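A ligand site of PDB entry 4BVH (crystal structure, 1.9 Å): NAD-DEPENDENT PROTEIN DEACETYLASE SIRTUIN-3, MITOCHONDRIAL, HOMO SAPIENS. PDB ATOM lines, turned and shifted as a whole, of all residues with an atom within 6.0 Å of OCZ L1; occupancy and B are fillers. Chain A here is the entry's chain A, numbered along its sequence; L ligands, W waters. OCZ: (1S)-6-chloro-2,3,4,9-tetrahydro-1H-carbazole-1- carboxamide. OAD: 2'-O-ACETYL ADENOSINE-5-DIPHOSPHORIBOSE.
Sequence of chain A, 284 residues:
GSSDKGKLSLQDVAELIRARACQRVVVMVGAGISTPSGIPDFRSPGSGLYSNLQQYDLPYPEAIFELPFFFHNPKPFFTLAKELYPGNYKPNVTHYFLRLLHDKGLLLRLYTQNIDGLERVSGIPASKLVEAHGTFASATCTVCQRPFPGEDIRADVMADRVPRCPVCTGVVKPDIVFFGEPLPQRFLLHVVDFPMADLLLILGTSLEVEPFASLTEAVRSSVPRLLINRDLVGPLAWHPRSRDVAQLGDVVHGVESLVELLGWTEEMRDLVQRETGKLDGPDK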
ATOM      1  N   GLY A  30     -14.841 -16.102  19.659  1.00  0.00           N
ATOM      2  CA  GLY A  30     -15.125 -16.383  18.241  1.00  0.00           C
ATOM      3  C   GLY A  30     -15.371 -15.096  17.446  1.00  0.00           C
ATOM      4  O   GLY A  30     -14.903 -13.982  17.800  1.00  0.00           O
ATOM      5  N   ALA A  31     -16.130 -15.245  16.357  1.00  0.00           N
ATOM      6  CA  ALA A  31     -16.146 -14.283  15.259  1.00  0.00           C
ATOM      7  C   ALA A  31     -16.829 -12.979  15.656  1.00  0.00           C
ATOM      8  O   ALA A  31     -16.604 -11.876  15.028  1.00  0.00           O
ATOM      9  CB  ALA A  31     -16.849 -14.931  14.078  1.00  0.00           C
ATOM     10  N   SER A  34     -14.790  -9.787  16.367  1.00  0.00           N
ATOM     11  CA  SER A  34     -14.142  -9.121  15.249  1.00  0.00           C
ATOM     12  C   SER A  34     -15.133  -8.392  14.323  1.00  0.00           C
ATOM     13  O   SER A  34     -14.718  -7.597  13.464  1.00  0.00           O
ATOM     14  CB  SER A  34     -13.256 -10.185  14.456  1.00  0.00           C
ATOM     15  OG  SER A  34     -12.170 -10.526  15.329  1.00  0.00           O
ATOM     16  N   ILE A  39     -15.145  -7.286  10.302  1.00  0.00           N
ATOM     17  CA  ILE A  39     -15.187  -8.639   9.742  1.00  0.00           C
ATOM     18  C   ILE A  39     -16.514  -9.283  10.076  1.00  0.00           C
ATOM     19  O   ILE A  39     -16.886  -9.402  11.252  1.00  0.00           O
ATOM     20  CB  ILE A  39     -13.997  -9.522  10.275  1.00  0.00           C
ATOM     21  CG1 ILE A  39     -12.661  -8.780  10.147  1.00  0.00           C
ATOM     22  CG2 ILE A  39     -13.974 -10.947   9.654  1.00  0.00           C
ATOM     23  CD1 ILE A  39     -11.514  -9.520  10.804  1.00  0.00           C
ATOM     24  N   PRO A  40     -17.277  -9.741   9.059  1.00  0.00           N
ATOM     25  CA  PRO A  40     -18.562 -10.376   9.393  1.00  0.00           C
ATOM     26  C   PRO A  40     -18.322 -11.660  10.225  1.00  0.00           C
ATOM     27  O   PRO A  40     -17.233 -12.210  10.138  1.00  0.00           O
ATOM     28  CB  PRO A  40     -19.145 -10.729   8.002  1.00  0.00           C
ATOM     29  CG  PRO A  40     -17.925 -10.844   7.132  1.00  0.00           C
ATOM     30  CD  PRO A  40     -16.914  -9.852   7.637  1.00  0.00           C
ATOM     31  N   ASP A  41     -19.313 -12.096  11.021  1.00  0.00           N
ATOM     32  CA  ASP A  41     -19.318 -13.423  11.621  1.00  0.00           C
ATOM     33  C   ASP A  41     -19.935 -14.470  10.704  1.00  0.00           C
ATOM     34  O   ASP A  41     -20.181 -14.176   9.556  1.00  0.00           O
ATOM     35  CB  ASP A  41     -19.993 -13.421  13.014  1.00  0.00           C
ATOM     36  CG  ASP A  41     -21.497 -13.119  12.969  1.00  0.00           C
ATOM     37  OD1 ASP A  41     -22.119 -13.141  11.874  1.00  0.00           O
ATOM     38  OD2 ASP A  41     -22.094 -12.885  14.067  1.00  0.00           O
ATOM     39  N   PHE A  42     -20.256 -15.627  11.223  1.00  0.00           N
ATOM     40  CA  PHE A  42     -20.954 -16.655  10.422  1.00  0.00           C
ATOM     41  C   PHE A  42     -22.461 -16.565  10.350  1.00  0.00           C
ATOM     42  O   PHE A  42     -23.036 -16.607   9.245  1.00  0.00           O
ATOM     43  CB  PHE A  42     -20.545 -18.075  10.802  1.00  0.00           C
ATOM     44  CG  PHE A  42     -19.094 -18.334  10.578  1.00  0.00           C
ATOM     45  CD1 PHE A  42     -18.638 -18.721   9.341  1.00  0.00           C
ATOM     46  CD2 PHE A  42     -18.185 -18.071  11.576  1.00  0.00           C
ATOM     47  CE1 PHE A  42     -17.285 -18.953   9.119  1.00  0.00           C
ATOM     48  CE2 PHE A  42     -16.822 -18.239  11.349  1.00  0.00           C
ATOM     49  CZ  PHE A  42     -16.380 -18.712  10.126  1.00  0.00           C
ATOM     50  N   LEU A  49     -21.609 -14.491   7.284  1.00  0.00           N
ATOM     51  CA  LEU A  49     -21.139 -15.198   6.079  1.00  0.00           C
ATOM     52  C   LEU A  49     -22.148 -16.197   5.561  1.00  0.00           C
ATOM     53  O   LEU A  49     -22.436 -16.243   4.363  1.00  0.00           O
ATOM     54  CB  LEU A  49     -19.778 -15.885   6.327  1.00  0.00           C
ATOM     55  CG  LEU A  49     -18.663 -14.833   6.440  1.00  0.00           C
ATOM     56  CD1 LEU A  49     -17.378 -15.411   7.091  1.00  0.00           C
ATOM     57  CD2 LEU A  49     -18.356 -14.165   5.105  1.00  0.00           C
ATOM     58  N   ILE A  64     -17.126 -23.536   1.686  1.00  0.00           N
ATOM     59  CA  ILE A  64     -15.965 -22.666   1.450  1.00  0.00           C
ATOM     60  C   ILE A  64     -14.857 -22.919   2.472  1.00  0.00           C
ATOM     61  O   ILE A  64     -13.684 -22.604   2.244  1.00  0.00           O
ATOM     62  CB  ILE A  64     -16.381 -21.175   1.404  1.00  0.00           C
ATOM     63  CG1 ILE A  64     -15.295 -20.326   0.723  1.00  0.00           C
ATOM     64  CG2 ILE A  64     -16.771 -20.625   2.776  1.00  0.00           C
ATOM     65  CD1 ILE A  64     -15.806 -19.057   0.074  1.00  0.00           C
ATOM     66  N   PHE A  65     -15.236 -23.470   3.604  1.00  0.00           N
ATOM     67  CA  PHE A  65     -14.287 -23.737   4.680  1.00  0.00           C
ATOM     68  C   PHE A  65     -14.105 -25.230   4.945  1.00  0.00           C
ATOM     69  O   PHE A  65     -13.700 -25.596   6.041  1.00  0.00           O
ATOM     70  CB  PHE A  65     -14.685 -22.982   5.956  1.00  0.00           C
ATOM     71  CG  PHE A  65     -14.762 -21.476   5.782  1.00  0.00           C
ATOM     72  CD1 PHE A  65     -13.663 -20.757   5.288  1.00  0.00           C
ATOM     73  CD2 PHE A  65     -15.920 -20.779   6.122  1.00  0.00           C
ATOM     74  CE1 PHE A  65     -13.709 -19.366   5.147  1.00  0.00           C
ATOM     75  CE2 PHE A  65     -15.979 -19.400   5.970  1.00  0.00           C
ATOM     76  CZ  PHE A  65     -14.870 -18.694   5.514  1.00  0.00           C
ATOM     77  N   PHE A  77     -12.655 -20.136  -1.801  1.00  0.00           N
ATOM     78  CA  PHE A  77     -11.868 -19.830  -0.601  1.00  0.00           C
ATOM     79  C   PHE A  77     -10.865 -18.691  -0.830  1.00  0.00           C
ATOM     80  O   PHE A  77     -10.896 -17.714  -0.097  1.00  0.00           O
ATOM     81  CB  PHE A  77     -11.170 -21.055   0.024  1.00  0.00           C
ATOM     82  CG  PHE A  77     -10.228 -20.670   1.109  1.00  0.00           C
ATOM     83  CD1 PHE A  77     -10.699 -20.432   2.406  1.00  0.00           C
ATOM     84  CD2 PHE A  77      -8.877 -20.422   0.820  1.00  0.00           C
ATOM     85  CE1 PHE A  77      -9.819 -20.030   3.414  1.00  0.00           C
ATOM     86  CE2 PHE A  77      -8.008 -20.002   1.803  1.00  0.00           C
ATOM     87  CZ  PHE A  77      -8.478 -19.829   3.115  1.00  0.00           C
ATOM     88  N   LEU A  84     -10.190 -11.267   4.017  1.00  0.00           N
ATOM     89  CA  LEU A  84      -9.875 -11.793   5.366  1.00  0.00           C
ATOM     90  C   LEU A  84      -8.406 -11.823   5.711  1.00  0.00           C
ATOM     91  O   LEU A  84      -8.087 -12.013   6.873  1.00  0.00           O
ATOM     92  CB  LEU A  84     -10.418 -13.204   5.580  1.00  0.00           C
ATOM     93  CG  LEU A  84     -11.812 -13.558   5.061  1.00  0.00           C
ATOM     94  CD1 LEU A  84     -12.024 -15.075   5.014  1.00  0.00           C
ATOM     95  CD2 LEU A  84     -12.866 -12.859   5.903  1.00  0.00           C
ATOM     96  N   GLN A 113     -11.235 -19.168  18.047  1.00  0.00           N
ATOM     97  CA  GLN A 113     -11.737 -19.839  16.843  1.00  0.00           C
ATOM     98  C   GLN A 113     -11.470 -19.050  15.565  1.00  0.00           C
ATOM     99  O   GLN A 113     -11.668 -19.562  14.451  1.00  0.00           O
ATOM    100  CB  GLN A 113     -13.263 -20.032  16.955  1.00  0.00           C
ATOM    101  CG  GLN A 113     -13.616 -21.009  18.092  1.00  0.00           C
ATOM    102  CD  GLN A 113     -15.096 -20.969  18.445  1.00  0.00           C
ATOM    103  OE1 GLN A 113     -15.853 -21.831  18.023  1.00  0.00           O
ATOM    104  NE2 GLN A 113     -15.515 -19.953  19.199  1.00  0.00           N
ATOM    105  N   ASN A 114     -11.092 -17.781  15.712  1.00  0.00           N
ATOM    106  CA  ASN A 114     -10.897 -16.889  14.560  1.00  0.00           C
ATOM    107  C   ASN A 114      -9.596 -17.157  13.816  1.00  0.00           C
ATOM    108  O   ASN A 114      -8.589 -17.574  14.427  1.00  0.00           O
ATOM    109  CB  ASN A 114     -10.911 -15.423  15.060  1.00  0.00           C
ATOM    110  CG  ASN A 114     -12.241 -15.045  15.687  1.00  0.00           C
ATOM    111  OD1 ASN A 114     -13.216 -15.767  15.483  1.00  0.00           O
ATOM    112  ND2 ASN A 114     -12.315 -13.919  16.418  1.00  0.00           N
ATOM    113  N   ILE A 115      -9.631 -16.927  12.484  1.00  0.00           N
ATOM    114  CA  ILE A 115      -8.412 -16.980  11.641  1.00  0.00           C
ATOM    115  C   ILE A 115      -7.919 -15.597  11.277  1.00  0.00           C
ATOM    116  O   ILE A 115      -6.955 -15.503  10.558  1.00  0.00           O
ATOM    117  CB  ILE A 115      -8.606 -17.854  10.367  1.00  0.00           C
ATOM    118  CG1 ILE A 115      -9.728 -17.272   9.496  1.00  0.00           C
ATOM    119  CG2 ILE A 115      -8.934 -19.280  10.798  1.00  0.00           C
ATOM    120  CD1 ILE A 115      -9.806 -17.891   8.107  1.00  0.00           C
ATOM    121  N   ASP A 116      -8.572 -14.530  11.780  1.00  0.00           N
ATOM    122  CA  ASP A 116      -8.184 -13.150  11.368  1.00  0.00           C
ATOM    123  C   ASP A 116      -6.834 -12.727  11.968  1.00  0.00           C
ATOM    124  O   ASP A 116      -6.265 -11.695  11.588  1.00  0.00           O
ATOM    125  CB  ASP A 116      -9.319 -12.150  11.726  1.00  0.00           C
ATOM    126  CG  ASP A 116      -9.679 -12.145  13.252  1.00  0.00           C
ATOM    127  OD1 ASP A 116      -8.776 -12.227  14.135  1.00  0.00           O
ATOM    128  OD2 ASP A 116     -10.898 -12.095  13.541  1.00  0.00           O
ATOM    129  N   GLY A 117      -6.345 -13.480  12.971  1.00  0.00           N
ATOM    130  CA  GLY A 117      -5.045 -13.194  13.567  1.00  0.00           C
ATOM    131  C   GLY A 117      -4.952 -11.949  14.464  1.00  0.00           C
ATOM    132  O   GLY A 117      -3.860 -11.510  14.819  1.00  0.00           O
ATOM    133  N   HIS A 133      -8.164 -22.680  15.124  1.00  0.00           N
ATOM    134  CA  HIS A 133      -8.404 -22.912  13.665  1.00  0.00           C
ATOM    135  C   HIS A 133      -7.257 -22.499  12.769  1.00  0.00           C
ATOM    136  O   HIS A 133      -7.414 -22.240  11.584  1.00  0.00           O
ATOM    137  CB  HIS A 133      -9.732 -22.269  13.253  1.00  0.00           C
ATOM    138  CG  HIS A 133     -10.908 -22.947  13.853  1.00  0.00           C
ATOM    139  ND1 HIS A 133     -12.032 -22.282  14.313  1.00  0.00           N
ATOM    140  CD2 HIS A 133     -11.123 -24.266  14.098  1.00  0.00           C
ATOM    141  CE1 HIS A 133     -12.894 -23.153  14.808  1.00  0.00           C
ATOM    142  NE2 HIS A 133     -12.345 -24.361  14.728  1.00  0.00           N
ATOM    143  N   ILE A 176      -4.797 -22.966   7.901  1.00  0.00           N
ATOM    144  CA  ILE A 176      -6.147 -22.837   8.469  1.00  0.00           C
ATOM    145  C   ILE A 176      -6.768 -24.209   8.619  1.00  0.00           C
ATOM    146  O   ILE A 176      -6.684 -25.030   7.708  1.00  0.00           O
ATOM    147  CB  ILE A 176      -7.051 -22.096   7.460  1.00  0.00           C
ATOM    148  CG1 ILE A 176      -6.580 -20.677   7.258  1.00  0.00           C
ATOM    149  CG2 ILE A 176      -8.506 -22.075   7.895  1.00  0.00           C
ATOM    150  CD1 ILE A 176      -6.200 -19.977   8.539  1.00  0.00           C
ATOM    151  N   VAL A 177      -7.428 -24.459   9.747  1.00  0.00           N
ATOM    152  CA  VAL A 177      -8.155 -25.681   9.956  1.00  0.00           C
ATOM    153  C   VAL A 177      -9.492 -25.568   9.288  1.00  0.00           C
ATOM    154  O   VAL A 177     -10.399 -24.867   9.754  1.00  0.00           O
ATOM    155  CB  VAL A 177      -8.364 -26.007  11.456  1.00  0.00           C
ATOM    156  CG1 VAL A 177      -8.927 -27.397  11.635  1.00  0.00           C
ATOM    157  CG2 VAL A 177      -7.019 -25.958  12.144  1.00  0.00           C
ATOM    158  N   PHE A 178      -9.603 -26.261   8.166  1.00  0.00           N
ATOM    159  CA  PHE A 178     -10.870 -26.434   7.473  1.00  0.00           C
ATOM    160  C   PHE A 178     -11.754 -27.418   8.246  1.00  0.00           C
ATOM    161  O   PHE A 178     -11.256 -28.157   9.101  1.00  0.00           O
ATOM    162  CB  PHE A 178     -10.604 -26.880   6.016  1.00  0.00           C
ATOM    163  CG  PHE A 178     -10.256 -25.738   5.084  1.00  0.00           C
ATOM    164  CD1 PHE A 178     -10.348 -24.417   5.496  1.00  0.00           C
ATOM    165  CD2 PHE A 178      -9.931 -25.985   3.768  1.00  0.00           C
ATOM    166  CE1 PHE A 178     -10.056 -23.376   4.636  1.00  0.00           C
ATOM    167  CE2 PHE A 178      -9.646 -24.950   2.903  1.00  0.00           C
ATOM    168  CZ  PHE A 178      -9.701 -23.636   3.337  1.00  0.00           C
ATOM    169  N   PHE A 179     -13.057 -27.401   7.954  1.00  0.00           N
ATOM    170  CA  PHE A 179     -14.042 -28.344   8.525  1.00  0.00           C
ATOM    171  C   PHE A 179     -13.598 -29.779   8.414  1.00  0.00           C
ATOM    172  O   PHE A 179     -13.087 -30.228   7.360  1.00  0.00           O
ATOM    173  CB  PHE A 179     -15.400 -28.240   7.835  1.00  0.00           C
ATOM    174  CG  PHE A 179     -16.352 -27.273   8.479  1.00  0.00           C
ATOM    175  CD1 PHE A 179     -16.650 -27.358   9.841  1.00  0.00           C
ATOM    176  CD2 PHE A 179     -16.990 -26.284   7.719  1.00  0.00           C
ATOM    177  CE1 PHE A 179     -17.534 -26.466  10.441  1.00  0.00           C
ATOM    178  CE2 PHE A 179     -17.874 -25.393   8.318  1.00  0.00           C
ATOM    179  CZ  PHE A 179     -18.154 -25.486   9.671  1.00  0.00           C
HETATM  180  NAQ OCZ L   1     -13.100 -13.519  12.339  1.00  0.00           N
HETATM  181  OAP OCZ L   1     -11.678 -15.160  11.868  1.00  0.00           O
HETATM  182  CAO OCZ L   1     -12.829 -14.734  11.795  1.00  0.00           C
HETATM  183  NAG OCZ L   1     -13.168 -17.994  11.777  1.00  0.00           N
HETATM  184  CAJ OCZ L   1     -13.620 -16.564   8.499  1.00  0.00           C
HETATM  185  CAD OCZ L   1     -12.456 -20.353  11.355  1.00  0.00           C
HETATM  186  CAC OCZ L   1     -12.137 -21.308  10.414  1.00  0.00           C
HETATM  187  CAE OCZ L   1     -12.826 -19.065  11.017  1.00  0.00           C
HETATM  188 CL   OCZ L   1     -11.804 -22.069   7.709  1.00  0.00          CL
HETATM  189  CAF OCZ L   1     -12.956 -18.698   9.729  1.00  0.00           C
HETATM  190  CAA OCZ L   1     -12.640 -19.600   8.771  1.00  0.00           C
HETATM  191  CAH OCZ L   1     -13.364 -17.385   9.665  1.00  0.00           C
HETATM  192  CAI OCZ L   1     -13.520 -16.928  10.964  1.00  0.00           C
HETATM  193  CAB OCZ L   1     -12.232 -20.906   9.090  1.00  0.00           C
HETATM  194  CAM OCZ L   1     -13.765 -14.999   8.838  1.00  0.00           C
HETATM  195  CAK OCZ L   1     -13.949 -15.558  11.318  1.00  0.00           C
HETATM  196  CAL OCZ L   1     -14.713 -14.862  10.110  1.00  0.00           C
HETATM  197  PA  OAD L   2     -20.658 -17.418  14.909  1.00  0.00           P
HETATM  198  O1A OAD L   2     -21.245 -18.859  14.867  1.00  0.00           O
HETATM  199  O2A OAD L   2     -20.845 -16.491  13.739  1.00  0.00           O
HETATM  200  O5' OAD L   2     -21.040 -16.769  16.345  1.00  0.00           O
HETATM  201  C5' OAD L   2     -20.827 -15.315  16.507  1.00  0.00           C
HETATM  202  C4' OAD L   2     -21.486 -14.916  17.867  1.00  0.00           C
HETATM  203  O4' OAD L   2     -21.183 -13.541  18.122  1.00  0.00           O
HETATM  204  C3' OAD L   2     -22.981 -14.991  17.653  1.00  0.00           C
HETATM  205  O3' OAD L   2     -23.583 -15.517  18.759  1.00  0.00           O
HETATM  206  C2' OAD L   2     -23.359 -13.534  17.361  1.00  0.00           C
HETATM  207  O2' OAD L   2     -24.712 -13.235  17.881  1.00  0.00           O
HETATM  208  C1' OAD L   2     -22.350 -12.775  18.296  1.00  0.00           C
HETATM  209  N9  OAD L   2     -21.977 -11.454  17.855  1.00  0.00           N
HETATM  210  C8  OAD L   2     -21.548 -11.036  16.633  1.00  0.00           C
HETATM  211  N7  OAD L   2     -21.314  -9.771  16.719  1.00  0.00           N
HETATM  212  C5  OAD L   2     -21.505  -9.332  17.968  1.00  0.00           C
HETATM  213  C6  OAD L   2     -21.361  -8.133  18.562  1.00  0.00           C
HETATM  214  N6  OAD L   2     -20.936  -7.077  17.866  1.00  0.00           N
HETATM  215  N1  OAD L   2     -21.629  -7.960  19.895  1.00  0.00           N
HETATM  216  C2  OAD L   2     -22.074  -9.031  20.627  1.00  0.00           C
HETATM  217  N3  OAD L   2     -22.187 -10.253  20.008  1.00  0.00           N
HETATM  218  C4  OAD L   2     -21.885 -10.381  18.682  1.00  0.00           C
HETATM  219  O3A OAD L   2     -19.018 -17.532  15.045  1.00  0.00           O
HETATM  220  PB  OAD L   2     -18.169 -18.492  15.946  1.00  0.00           P
HETATM  221  O1B OAD L   2     -18.854 -18.973  17.194  1.00  0.00           O
HETATM  222  O2B OAD L   2     -16.765 -18.021  15.990  1.00  0.00           O
HETATM  223  O2D OAD L   2     -15.145 -22.618  11.948  1.00  0.00           O
HETATM  224  O5D OAD L   2     -18.247 -19.791  14.951  1.00  0.00           O
HETATM  225  C5D OAD L   2     -17.368 -20.853  15.315  1.00  0.00           C
HETATM  226  C4D OAD L   2     -16.897 -21.556  14.069  1.00  0.00           C
HETATM  227  O4D OAD L   2     -18.049 -21.746  13.208  1.00  0.00           O
HETATM  228  C3D OAD L   2     -15.951 -20.698  13.205  1.00  0.00           C
HETATM  229  O3D OAD L   2     -14.578 -20.551  13.749  1.00  0.00           O
HETATM  230  C2D OAD L   2     -16.024 -21.493  11.852  1.00  0.00           C
HETATM  231  C1D OAD L   2     -17.553 -21.851  11.836  1.00  0.00           C
HETATM  232  O1D OAD L   2     -17.805 -23.232  11.519  1.00  0.00           O
HETATM  233  C6D OAD L   2     -14.968 -23.588  10.991  1.00  0.00           C
HETATM  234  O6D OAD L   2     -14.554 -24.726  11.272  1.00  0.00           O
HETATM  235  C7D OAD L   2     -15.231 -23.187   9.541  1.00  0.00           C
HETATM  236  O   HOH W   1     -14.439 -17.831  14.412  1.00  0.00           O
HETATM  237  O   HOH W   2     -15.433 -11.976  12.517  1.00  0.00           O
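Water W1 lies within hydrogen-bond range of the side-chain amide oxygen (OD1) of Asn 114 (2.6 Å), an oxygen (O3D) of OAD L2 (2.8 Å), a nitrogen (NAG) of OCZ L1 (2.9 Å) and the backbone carbonyl oxygen (O) of Gln 113 (3.3 Å).
Merely in contact with OCZ L1: Ser 34 (3.95 Å), Ile 39 (3.8 Å), Pro 40 (3.7 Å), Phe 42 (3.3 Å), Phe 65 (3.3 Å), Leu 84 (3.7 Å), Asn 114 (3.3 Å), His 133 (3.6 Å), Ile 176 (3.3 Å), Val 177 (3.7 Å) and Phe 178 (3.5 Å).
An oxygen (O3D) of OAD L2 is in hydrogen-bond range of a ring nitrogen (ND1) of His 133, at 3.1 Å.
OD2 of Asp 116 sits at hydrogen-bond distance from NAQ of OCZ L1 (2.9 Å).
The backbone carbonyl oxygen of Gln 113 sits close to a nitrogen (NAG) of OCZ L1 (3.4 Å).
An oxygen (O2A) of OAD L2 is in hydrogen-bond range of the backbone NH (N) of Phe 42 (2.7 Å).
The backbone NH (N) of Ala 31 lies within hydrogen-bond range of an oxygen (O2B) of OAD L2 (2.9 Å).
The backbone NH of Ile 115 lies within hydrogen-bond range of an oxygen (OAP) of OCZ L1 (2.8 Å).
An oxygen (OAP) of OCZ L1 lies within hydrogen-bond range of the backbone NH of Asp 116 (3.2 Å).
O of Gln 113 is in hydrogen-bond range of O3D of OAD L2 (3.2 Å).
The side-chain amide nitrogen (ND2) of Asn 114 is in hydrogen-bond range of the backbone carbonyl oxygen (O) of Gly 30, at 2.9 Å.
The backbone carbonyl oxygen (O) of His 133 is in hydrogen-bond range of the backbone NH (N) of Val 177 (2.9 Å).
O of Phe 42 is in hydrogen-bond range of N of Leu 49, 3.2 Å away.
The backbone NH (N) of Ile 39 sits at hydrogen-bond distance from the backbone carbonyl oxygen (O) of Ser 34.
O of Gln 113 is in hydrogen-bond range of ND1 of His 133, at 2.7 Å.
The backbone carbonyl oxygen (O) of Phe 65 lies within hydrogen-bond range of the backbone NH (N) of Phe 179, 2.7 Å away.
The side-chain carboxylate (OD2) of Asp 116 sits at hydrogen-bond distance from the side-chain hydroxyl (OG) of Ser 34, at 2.7 Å.
The side-chain amide oxygen (OD1) of Asn 114 sits at hydrogen-bond distance from the backbone NH (N) of Ala 31, at 3.1 Å.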
